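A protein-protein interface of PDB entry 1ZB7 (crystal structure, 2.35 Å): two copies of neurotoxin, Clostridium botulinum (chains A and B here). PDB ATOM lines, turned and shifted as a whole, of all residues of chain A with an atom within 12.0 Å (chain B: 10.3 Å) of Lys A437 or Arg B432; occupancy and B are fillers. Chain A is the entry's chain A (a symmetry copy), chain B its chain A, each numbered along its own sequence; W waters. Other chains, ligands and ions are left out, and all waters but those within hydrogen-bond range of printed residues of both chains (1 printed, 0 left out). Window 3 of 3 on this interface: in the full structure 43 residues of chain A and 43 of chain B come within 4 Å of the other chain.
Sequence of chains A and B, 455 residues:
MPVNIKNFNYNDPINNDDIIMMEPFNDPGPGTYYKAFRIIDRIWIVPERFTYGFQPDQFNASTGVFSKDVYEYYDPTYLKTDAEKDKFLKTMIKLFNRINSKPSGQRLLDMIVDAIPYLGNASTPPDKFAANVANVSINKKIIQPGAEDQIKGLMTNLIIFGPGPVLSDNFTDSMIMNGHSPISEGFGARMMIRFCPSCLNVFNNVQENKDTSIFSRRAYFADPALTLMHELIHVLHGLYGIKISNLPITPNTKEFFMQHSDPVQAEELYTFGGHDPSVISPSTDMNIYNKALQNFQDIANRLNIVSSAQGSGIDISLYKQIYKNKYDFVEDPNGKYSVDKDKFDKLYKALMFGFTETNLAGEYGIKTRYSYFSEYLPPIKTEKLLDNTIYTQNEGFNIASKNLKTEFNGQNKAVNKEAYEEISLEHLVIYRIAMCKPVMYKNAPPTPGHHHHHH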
ATOM      1  N   PHE A 257     -10.058   2.579  12.032  1.00  0.00           N
ATOM      2  CA  PHE A 257      -9.019   3.629  11.936  1.00  0.00           C
ATOM      3  C   PHE A 257      -8.033   3.702  13.167  1.00  0.00           C
ATOM      4  O   PHE A 257      -8.268   3.170  14.268  1.00  0.00           O
ATOM      5  CB  PHE A 257      -9.585   5.046  11.471  1.00  0.00           C
ATOM      6  CG  PHE A 257     -10.274   5.884  12.574  1.00  0.00           C
ATOM      7  CD1 PHE A 257      -9.588   6.922  13.220  1.00  0.00           C
ATOM      8  CD2 PHE A 257     -11.607   5.639  12.944  1.00  0.00           C
ATOM      9  CE1 PHE A 257     -10.198   7.669  14.245  1.00  0.00           C
ATOM     10  CE2 PHE A 257     -12.229   6.401  13.928  1.00  0.00           C
ATOM     11  CZ  PHE A 257     -11.512   7.425  14.595  1.00  0.00           C
ATOM     12  N   MET A 258      -6.919   4.389  12.894  1.00  0.00           N
ATOM     13  CA  MET A 258      -5.743   4.472  13.742  1.00  0.00           C
ATOM     14  C   MET A 258      -5.619   5.919  14.264  1.00  0.00           C
ATOM     15  O   MET A 258      -5.649   6.873  13.483  1.00  0.00           O
ATOM     16  CB  MET A 258      -4.515   4.053  12.925  1.00  0.00           C
ATOM     17  CG  MET A 258      -4.462   4.604  11.442  1.00  0.00           C
ATOM     18  SD  MET A 258      -5.800   4.282  10.184  1.00  0.00           S
ATOM     19  CE  MET A 258      -5.861   2.489  10.039  1.00  0.00           C
ATOM     20  N   GLN A 259      -5.550   6.047  15.596  1.00  0.00           N
ATOM     21  CA  GLN A 259      -5.442   7.327  16.308  1.00  0.00           C
ATOM     22  C   GLN A 259      -4.391   8.211  15.682  1.00  0.00           C
ATOM     23  O   GLN A 259      -3.379   7.723  15.218  1.00  0.00           O
ATOM     24  CB  GLN A 259      -5.137   7.086  17.788  1.00  0.00           C
ATOM     25  CG  GLN A 259      -4.661   8.285  18.554  1.00  0.00           C
ATOM     26  CD  GLN A 259      -4.983   8.212  20.062  1.00  0.00           C
ATOM     27  OE1 GLN A 259      -5.537   7.240  20.561  1.00  0.00           O
ATOM     28  NE2 GLN A 259      -4.671   9.269  20.761  1.00  0.00           N
ATOM     29  N   HIS A 260      -4.670   9.509  15.614  1.00  0.00           N
ATOM     30  CA  HIS A 260      -3.741  10.492  15.033  1.00  0.00           C
ATOM     31  C   HIS A 260      -4.183  11.874  15.400  1.00  0.00           C
ATOM     32  O   HIS A 260      -5.277  12.060  15.975  1.00  0.00           O
ATOM     33  CB  HIS A 260      -3.642  10.386  13.522  1.00  0.00           C
ATOM     34  CG  HIS A 260      -4.917  10.735  12.803  1.00  0.00           C
ATOM     35  ND1 HIS A 260      -5.188  12.011  12.346  1.00  0.00           N
ATOM     36  CD2 HIS A 260      -5.997   9.974  12.470  1.00  0.00           C
ATOM     37  CE1 HIS A 260      -6.372  12.014  11.759  1.00  0.00           C
ATOM     38  NE2 HIS A 260      -6.888  10.797  11.826  1.00  0.00           N
ATOM     39  N   SER A 261      -3.310  12.842  15.128  1.00  0.00           N
ATOM     40  CA  SER A 261      -3.569  14.194  15.563  1.00  0.00           C
ATOM     41  C   SER A 261      -4.339  14.979  14.489  1.00  0.00           C
ATOM     42  O   SER A 261      -4.263  14.688  13.273  1.00  0.00           O
ATOM     43  CB  SER A 261      -2.280  14.904  16.020  1.00  0.00           C
ATOM     44  OG  SER A 261      -1.399  15.126  14.957  1.00  0.00           O
ATOM     45  N   PRO A 263      -5.025  17.517  11.809  1.00  0.00           N
ATOM     46  CA  PRO A 263      -4.175  18.306  10.897  1.00  0.00           C
ATOM     47  C   PRO A 263      -4.204  19.796  11.179  1.00  0.00           C
ATOM     48  O   PRO A 263      -3.226  20.482  10.924  1.00  0.00           O
ATOM     49  CB  PRO A 263      -4.777  18.025   9.506  1.00  0.00           C
ATOM     50  CG  PRO A 263      -5.442  16.701   9.689  1.00  0.00           C
ATOM     51  CD  PRO A 263      -6.006  16.706  11.064  1.00  0.00           C
ATOM     52  N   TYR A 431      10.134  17.333  -3.457  1.00  0.00           N
ATOM     53  CA  TYR A 431       9.196  16.232  -3.300  1.00  0.00           C
ATOM     54  C   TYR A 431       7.782  16.580  -3.713  1.00  0.00           C
ATOM     55  O   TYR A 431       7.349  17.730  -3.578  1.00  0.00           O
ATOM     56  CB  TYR A 431       9.081  15.857  -1.827  1.00  0.00           C
ATOM     57  CG  TYR A 431      10.340  15.458  -1.159  1.00  0.00           C
ATOM     58  CD1 TYR A 431      10.651  14.124  -0.992  1.00  0.00           C
ATOM     59  CD2 TYR A 431      11.188  16.414  -0.595  1.00  0.00           C
ATOM     60  CE1 TYR A 431      11.809  13.750  -0.286  1.00  0.00           C
ATOM     61  CE2 TYR A 431      12.348  16.057   0.048  1.00  0.00           C
ATOM     62  CZ  TYR A 431      12.647  14.722   0.229  1.00  0.00           C
ATOM     63  OH  TYR A 431      13.772  14.350   0.905  1.00  0.00           O
ATOM     64  N   ARG A 432       7.042  15.558  -4.112  1.00  0.00           N
ATOM     65  CA  ARG A 432       5.601  15.696  -4.313  1.00  0.00           C
ATOM     66  C   ARG A 432       4.841  14.837  -3.330  1.00  0.00           C
ATOM     67  O   ARG A 432       5.329  13.834  -2.842  1.00  0.00           O
ATOM     68  CB  ARG A 432       5.153  15.515  -5.778  1.00  0.00           C
ATOM     69  CG  ARG A 432       5.708  14.366  -6.533  1.00  0.00           C
ATOM     70  CD  ARG A 432       4.820  13.087  -6.414  1.00  0.00           C
ATOM     71  NE  ARG A 432       5.434  11.970  -7.161  1.00  0.00           N
ATOM     72  CZ  ARG A 432       5.397  10.702  -6.793  1.00  0.00           C
ATOM     73  NH1 ARG A 432       4.765  10.380  -5.699  1.00  0.00           N
ATOM     74  NH2 ARG A 432       5.994   9.768  -7.512  1.00  0.00           N
ATOM     75  N   ILE A 433       3.699  15.359  -2.926  1.00  0.00           N
ATOM     76  CA  ILE A 433       2.830  14.696  -1.985  1.00  0.00           C
ATOM     77  C   ILE A 433       2.191  13.459  -2.727  1.00  0.00           C
ATOM     78  O   ILE A 433       1.784  13.574  -3.830  1.00  0.00           O
ATOM     79  CB  ILE A 433       1.834  15.726  -1.378  1.00  0.00           C
ATOM     80  CG1 ILE A 433       2.195  16.028   0.074  1.00  0.00           C
ATOM     81  CG2 ILE A 433       0.414  15.174  -1.338  1.00  0.00           C
ATOM     82  CD1 ILE A 433       3.697  16.631   0.342  1.00  0.00           C
ATOM     83  N   ALA A 434       2.255  12.275  -2.133  1.00  0.00           N
ATOM     84  CA  ALA A 434       1.718  11.055  -2.723  1.00  0.00           C
ATOM     85  C   ALA A 434       0.820  10.325  -1.684  1.00  0.00           C
ATOM     86  O   ALA A 434       0.907  10.573  -0.511  1.00  0.00           O
ATOM     87  CB  ALA A 434       2.847  10.154  -3.226  1.00  0.00           C
ATOM     88  N   MET A 435      -0.060   9.448  -2.148  1.00  0.00           N
ATOM     89  CA  MET A 435      -0.865   8.586  -1.256  1.00  0.00           C
ATOM     90  C   MET A 435      -0.254   7.197  -1.346  1.00  0.00           C
ATOM     91  O   MET A 435      -0.149   6.655  -2.443  1.00  0.00           O
ATOM     92  CB  MET A 435      -2.325   8.455  -1.716  1.00  0.00           C
ATOM     93  CG  MET A 435      -3.143   9.733  -1.931  1.00  0.00           C
ATOM     94  SD  MET A 435      -4.726   9.349  -2.902  1.00  0.00           S
ATOM     95  CE  MET A 435      -5.703  10.764  -2.233  1.00  0.00           C
ATOM     96  N   CYS A 436       0.177   6.652  -0.217  1.00  0.00           N
ATOM     97  CA  CYS A 436       0.925   5.396  -0.198  1.00  0.00           C
ATOM     98  C   CYS A 436       0.359   4.427   0.813  1.00  0.00           C
ATOM     99  O   CYS A 436      -0.300   4.861   1.745  1.00  0.00           O
ATOM    100  CB  CYS A 436       2.367   5.710   0.164  1.00  0.00           C
ATOM    101  SG  CYS A 436       3.156   6.925  -1.003  1.00  0.00           S
ATOM    102  N   LYS A 437       0.605   3.136   0.634  1.00  0.00           N
ATOM    103  CA  LYS A 437       0.326   2.140   1.692  1.00  0.00           C
ATOM    104  C   LYS A 437       0.991   2.561   2.985  1.00  0.00           C
ATOM    105  O   LYS A 437       2.161   2.876   2.955  1.00  0.00           O
ATOM    106  CB  LYS A 437       0.873   0.783   1.311  1.00  0.00           C
ATOM    107  CG  LYS A 437      -0.156  -0.137   0.770  1.00  0.00           C
ATOM    108  CD  LYS A 437       0.468  -1.358   0.186  1.00  0.00           C
ATOM    109  CE  LYS A 437      -0.538  -2.478  -0.025  1.00  0.00           C
ATOM    110  NZ  LYS A 437      -1.076  -3.054   1.275  1.00  0.00           N
ATOM    111  N   PRO A 438       0.255   2.580   4.128  1.00  0.00           N
ATOM    112  CA  PRO A 438       0.832   2.897   5.452  1.00  0.00           C
ATOM    113  C   PRO A 438       1.781   1.807   6.019  1.00  0.00           C
ATOM    114  O   PRO A 438       1.828   0.691   5.448  1.00  0.00           O
ATOM    115  CB  PRO A 438      -0.412   3.054   6.349  1.00  0.00           C
ATOM    116  CG  PRO A 438      -1.468   2.267   5.678  1.00  0.00           C
ATOM    117  CD  PRO A 438      -1.174   2.205   4.225  1.00  0.00           C
ATOM    118  N   LYS B  68      -4.124  14.002   5.489  1.00  0.00           N
ATOM    119  CA  LYS B  68      -3.377  13.079   6.367  1.00  0.00           C
ATOM    120  C   LYS B  68      -3.523  11.563   6.067  1.00  0.00           C
ATOM    121  O   LYS B  68      -2.545  10.847   5.803  1.00  0.00           O
ATOM    122  N   ASP B  69      -4.753  11.087   6.190  1.00  0.00           N
ATOM    123  CA  ASP B  69      -5.135   9.701   5.895  1.00  0.00           C
ATOM    124  C   ASP B  69      -6.299   9.696   4.914  1.00  0.00           C
ATOM    125  O   ASP B  69      -7.012  10.667   4.796  1.00  0.00           O
ATOM    126  CB  ASP B  69      -5.557   9.000   7.159  1.00  0.00           C
ATOM    127  CG  ASP B  69      -4.406   8.388   7.893  1.00  0.00           C
ATOM    128  OD1 ASP B  69      -3.485   7.798   7.253  1.00  0.00           O
ATOM    129  OD2 ASP B  69      -4.452   8.475   9.128  1.00  0.00           O
ATOM    130  N   VAL B  70      -6.457   8.623   4.161  1.00  0.00           N
ATOM    131  CA  VAL B  70      -7.394   8.582   3.024  1.00  0.00           C
ATOM    132  C   VAL B  70      -7.983   7.149   2.955  1.00  0.00           C
ATOM    133  O   VAL B  70      -7.271   6.184   3.011  1.00  0.00           O
ATOM    134  CB  VAL B  70      -6.658   8.947   1.716  1.00  0.00           C
ATOM    135  CG1 VAL B  70      -7.543   8.866   0.467  1.00  0.00           C
ATOM    136  CG2 VAL B  70      -6.088  10.320   1.810  1.00  0.00           C
ATOM    137  N   TYR B  71      -9.292   7.070   2.821  1.00  0.00           N
ATOM    138  CA  TYR B  71     -10.052   5.818   2.773  1.00  0.00           C
ATOM    139  C   TYR B  71     -10.847   5.613   1.466  1.00  0.00           C
ATOM    140  O   TYR B  71     -11.850   6.231   1.311  1.00  0.00           O
ATOM    141  CB  TYR B  71     -11.033   5.865   3.916  1.00  0.00           C
ATOM    142  CG  TYR B  71     -10.329   6.198   5.191  1.00  0.00           C
ATOM    143  CD1 TYR B  71      -9.537   5.246   5.833  1.00  0.00           C
ATOM    144  CD2 TYR B  71     -10.389   7.490   5.712  1.00  0.00           C
ATOM    145  CE1 TYR B  71      -8.838   5.559   7.031  1.00  0.00           C
ATOM    146  CE2 TYR B  71      -9.704   7.830   6.886  1.00  0.00           C
ATOM    147  CZ  TYR B  71      -8.925   6.872   7.532  1.00  0.00           C
ATOM    148  OH  TYR B  71      -8.277   7.278   8.667  1.00  0.00           O
ATOM    149  N   GLU B  72     -10.395   4.735   0.566  1.00  0.00           N
ATOM    150  CA  GLU B  72     -11.124   4.363  -0.626  1.00  0.00           C
ATOM    151  C   GLU B  72     -12.037   3.138  -0.321  1.00  0.00           C
ATOM    152  O   GLU B  72     -11.578   2.067   0.064  1.00  0.00           O
ATOM    153  CB  GLU B  72     -10.150   4.043  -1.765  1.00  0.00           C
ATOM    154  CG  GLU B  72      -9.285   5.213  -2.182  1.00  0.00           C
ATOM    155  CD  GLU B  72      -8.575   4.977  -3.496  1.00  0.00           C
ATOM    156  OE1 GLU B  72      -8.053   3.845  -3.809  1.00  0.00           O
ATOM    157  OE2 GLU B  72      -8.554   5.952  -4.248  1.00  0.00           O
ATOM    158  N   LEU B 425     -12.852  -3.982   6.363  1.00  0.00           N
ATOM    159  CA  LEU B 425     -11.556  -3.935   5.723  1.00  0.00           C
ATOM    160  C   LEU B 425     -11.439  -4.696   4.428  1.00  0.00           C
ATOM    161  O   LEU B 425     -10.526  -4.452   3.624  1.00  0.00           O
ATOM    162  CB  LEU B 425     -10.490  -4.469   6.704  1.00  0.00           C
ATOM    163  CG  LEU B 425     -10.012  -3.434   7.731  1.00  0.00           C
ATOM    164  CD1 LEU B 425      -8.856  -4.073   8.532  1.00  0.00           C
ATOM    165  CD2 LEU B 425      -9.592  -2.076   7.083  1.00  0.00           C
ATOM    166  N   LEU B 428     -12.210  -1.613   2.261  1.00  0.00           N
ATOM    167  CA  LEU B 428     -11.712  -0.279   2.576  1.00  0.00           C
ATOM    168  C   LEU B 428     -10.215  -0.262   2.331  1.00  0.00           C
ATOM    169  O   LEU B 428      -9.570  -1.062   2.871  1.00  0.00           O
ATOM    170  CB  LEU B 428     -12.089   0.114   4.005  1.00  0.00           C
ATOM    171  CG  LEU B 428     -12.447   1.625   4.193  1.00  0.00           C
ATOM    172  CD1 LEU B 428     -13.477   2.149   3.315  1.00  0.00           C
ATOM    173  CD2 LEU B 428     -12.899   1.845   5.613  1.00  0.00           C
ATOM    174  N   VAL B 429      -9.734   0.513   1.333  1.00  0.00           N
ATOM    175  CA  VAL B 429      -8.289   0.625   1.064  1.00  0.00           C
ATOM    176  C   VAL B 429      -7.782   1.904   1.749  1.00  0.00           C
ATOM    177  O   VAL B 429      -8.355   2.987   1.578  1.00  0.00           O
ATOM    178  CB  VAL B 429      -7.952   0.684  -0.450  1.00  0.00           C
ATOM    179  CG1 VAL B 429      -6.391   0.590  -0.652  1.00  0.00           C
ATOM    180  CG2 VAL B 429      -8.643  -0.446  -1.193  1.00  0.00           C
ATOM    181  N   ILE B 430      -6.727   1.771   2.509  1.00  0.00           N
ATOM    182  CA  ILE B 430      -6.234   2.862   3.375  1.00  0.00           C
ATOM    183  C   ILE B 430      -4.880   3.399   2.830  1.00  0.00           C
ATOM    184  O   ILE B 430      -3.959   2.650   2.544  1.00  0.00           O
ATOM    185  CB  ILE B 430      -5.933   2.405   4.828  1.00  0.00           C
ATOM    186  CG1 ILE B 430      -7.029   1.513   5.412  1.00  0.00           C
ATOM    187  CG2 ILE B 430      -5.676   3.617   5.728  1.00  0.00           C
ATOM    188  CD1 ILE B 430      -8.350   2.186   5.621  1.00  0.00           C
ATOM    189  N   TYR B 431      -4.768   4.705   2.755  1.00  0.00           N
ATOM    190  CA  TYR B 431      -3.494   5.315   2.403  1.00  0.00           C
ATOM    191  C   TYR B 431      -3.047   6.384   3.377  1.00  0.00           C
ATOM    192  O   TYR B 431      -3.876   7.082   3.974  1.00  0.00           O
ATOM    193  CB  TYR B 431      -3.619   6.042   1.069  1.00  0.00           C
ATOM    194  CG  TYR B 431      -4.043   5.217  -0.083  1.00  0.00           C
ATOM    195  CD1 TYR B 431      -3.108   4.726  -0.972  1.00  0.00           C
ATOM    196  CD2 TYR B 431      -5.395   5.000  -0.355  1.00  0.00           C
ATOM    197  CE1 TYR B 431      -3.523   4.009  -2.110  1.00  0.00           C
ATOM    198  CE2 TYR B 431      -5.803   4.255  -1.432  1.00  0.00           C
ATOM    199  CZ  TYR B 431      -4.868   3.781  -2.330  1.00  0.00           C
ATOM    200  OH  TYR B 431      -5.259   3.077  -3.431  1.00  0.00           O
ATOM    201  N   ARG B 432      -1.739   6.574   3.446  1.00  0.00           N
ATOM    202  CA  ARG B 432      -1.175   7.721   4.156  1.00  0.00           C
ATOM    203  C   ARG B 432      -0.456   8.640   3.197  1.00  0.00           C
ATOM    204  O   ARG B 432       0.018   8.233   2.151  1.00  0.00           O
ATOM    205  CB  ARG B 432      -0.344   7.340   5.399  1.00  0.00           C
ATOM    206  CG  ARG B 432       0.638   6.238   5.263  1.00  0.00           C
ATOM    207  CD  ARG B 432       2.052   6.745   4.839  1.00  0.00           C
ATOM    208  NE  ARG B 432       2.980   5.605   4.693  1.00  0.00           N
ATOM    209  CZ  ARG B 432       3.940   5.519   3.789  1.00  0.00           C
ATOM    210  NH1 ARG B 432       4.116   6.509   2.960  1.00  0.00           N
ATOM    211  NH2 ARG B 432       4.711   4.449   3.715  1.00  0.00           N
ATOM    212  N   ILE B 433      -0.543   9.918   3.506  1.00  0.00           N
ATOM    213  CA  ILE B 433       0.071  10.954   2.713  1.00  0.00           C
ATOM    214  C   ILE B 433       1.631  10.842   2.921  1.00  0.00           C
ATOM    215  O   ILE B 433       2.075  10.673   4.002  1.00  0.00           O
ATOM    216  CB  ILE B 433      -0.573  12.328   3.057  1.00  0.00           C
ATOM    217  CG1 ILE B 433      -1.464  12.803   1.912  1.00  0.00           C
ATOM    218  CG2 ILE B 433       0.483  13.415   3.228  1.00  0.00           C
ATOM    219  CD1 ILE B 433      -2.700  11.811   1.490  1.00  0.00           C
ATOM    220  N   ALA B 434       2.403  10.802   1.843  1.00  0.00           N
ATOM    221  CA  ALA B 434       3.854  10.682   1.902  1.00  0.00           C
ATOM    222  C   ALA B 434       4.505  11.775   1.007  1.00  0.00           C
ATOM    223  O   ALA B 434       3.868  12.332   0.152  1.00  0.00           O
ATOM    224  CB  ALA B 434       4.299   9.277   1.493  1.00  0.00           C
ATOM    225  N   MET B 435       5.771  12.085   1.245  1.00  0.00           N
ATOM    226  CA  MET B 435       6.542  12.997   0.374  1.00  0.00           C
ATOM    227  C   MET B 435       7.481  12.115  -0.435  1.00  0.00           C
ATOM    228  O   MET B 435       8.258  11.366   0.151  1.00  0.00           O
ATOM    229  CB  MET B 435       7.428  13.971   1.167  1.00  0.00           C
ATOM    230  CG  MET B 435       6.772  14.851   2.236  1.00  0.00           C
ATOM    231  SD  MET B 435       8.092  15.620   3.360  1.00  0.00           S
ATOM    232  CE  MET B 435       7.096  17.097   3.836  1.00  0.00           C
ATOM    233  N   CYS B 436       7.380  12.177  -1.755  1.00  0.00           N
ATOM    234  CA  CYS B 436       8.112  11.265  -2.632  1.00  0.00           C
ATOM    235  C   CYS B 436       8.831  12.009  -3.732  1.00  0.00           C
ATOM    236  O   CYS B 436       8.436  13.119  -4.053  1.00  0.00           O
ATOM    237  CB  CYS B 436       7.113  10.301  -3.251  1.00  0.00           C
ATOM    238  SG  CYS B 436       6.143   9.351  -1.979  1.00  0.00           S
HETATM  239  O   HOH W   1      -4.377   7.571  11.407  1.00  0.00           O
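N of Arg B432 is in hydrogen-bond range of O of Cys A436 (2.8 Å).
The backbone carbonyl oxygen (O) of Lys A437 sits at hydrogen-bond distance from the guanidinium group (NH2) of Arg B432 (3.1 Å).
The backbone carbonyl oxygen (O) of Ala B434 sits at hydrogen-bond distance from the backbone NH (N) of Ala A434 (2.8 Å).
The backbone carbonyl oxygen (O) of Cys B436 lies within hydrogen-bond range of the backbone NH (N) of Arg A432, 2.8 Å away.
O of Lys B68 sits at hydrogen-bond distance from N of Ile B433 (3.2 Å).
The backbone carbonyl oxygen (O) of Val B70 lies within hydrogen-bond range of the backbone NH (N) of Tyr B431 (2.9 Å).
The side-chain hydroxyl (OH) of Tyr B431 is in hydrogen-bond range of the side-chain carboxylate (OE1) of Glu B72, 2.9 Å away.
Among the printed residues, merely in contact across the chains: Phe A257 with Tyr B71 (3.8 Å), His A260 with Asp B69 (3.98 Å), Tyr A431 with Met B435 (3.8 Å), Tyr A431 with Cys B436 (3.3 Å), Arg A432 with Ala B434 (3.7 Å), Arg A432 with Met B435 (3.5 Å), Ile A433 with Ala B434 (3.4 Å), Ala A434 with Arg B432 (3.7 Å), Ala A434 with Ile B433 (3.4 Å), Ala A434 with Cys B436 (3.6 Å), Met A435 with Val B70 (3.8 Å), Met A435 with Tyr B431 (3.8 Å), Met A435 with Arg B432 (3.5 Å), Cys A436 with Tyr B431 (3.3 Å), Cys A436 with Ala B434 (3.6 Å), Cys A436 with Cys B436 (3.97 Å), Pro A438 with Ile B430 (3.3 Å) and Pro A438 with Arg B432 (3.4 Å).
Lys A437 touches just one residue of chain B: Arg B432 (3.1 Å).
Printed residues of chain A within 4 Å of Arg B432: Ala A434 (3.7 Å), Met A435 (3.5 Å), Cys A436 (2.8 Å), Lys A437 (3.1 Å) and Pro A438 (3.4 Å).
Cys A436 touches just these residues of chain B: Tyr B431, Arg B432, Ala B434 and Cys B436.
Asp B69 touches just one residue of chain A: His A260.
Val B70 touches one residue of chain A.
Tyr B431 touches two residues of chain A.
Ile B433 touches just one residue of chain A: Ala A434.
Of chain A, only Arg A432 (3.7 Å), Ile A433 (3.4 Å), Ala A434 (2.8 Å) and Cys A436 (3.6 Å) come within 4 Å of Ala B434.
Of the printed residues of chain B, Arg A432 touches Ala B434, Met B435 and Cys B436.
Printed residues of chain B within 4 Å of Tyr A431: Met B435 (3.8 Å) and Cys B436 (3.3 Å).
Pro A263 touches none of the printed residues of chain B.
The nearest residue of chain B that does not touch Lys A437 is Tyr B431 (4.3 Å).
The nearest residue of chain A that does not touch Arg B432 is Ile A433 (7.5 Å).
Of the 15 printed residues of chain B, 10 touch a printed residue of chain A.
Along chain B the printed residues that touch a printed residue of chain A span positions 69 to 436.
Of the 14 printed residues of chain A, 10 touch a printed residue of chain B.
Hydrophobic or aromatic side chains of chain A that line the printed part of chain B: Phe A257, His A260, Tyr A431, Ala A434, Met A435 and Pro A438.
Arg A432 touches Met B435, and with the chains exchanged Met A435 touches Arg B432.
Ile A433 touches Ala B434, and with the chains exchanged Ala A434 touches Ile B433.
Ala A434 touches its own counterpart, Ala B434.
Ala A434 touches Cys B436, and with the chains exchanged Cys A436 touches Ala B434.
Positions printed for both chains: 431, 432, 433, 434, 435 and 436.
Water W1 bridges OD2 of Asp B69 (2.5 Å) and O of Met A258 (2.5 Å).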
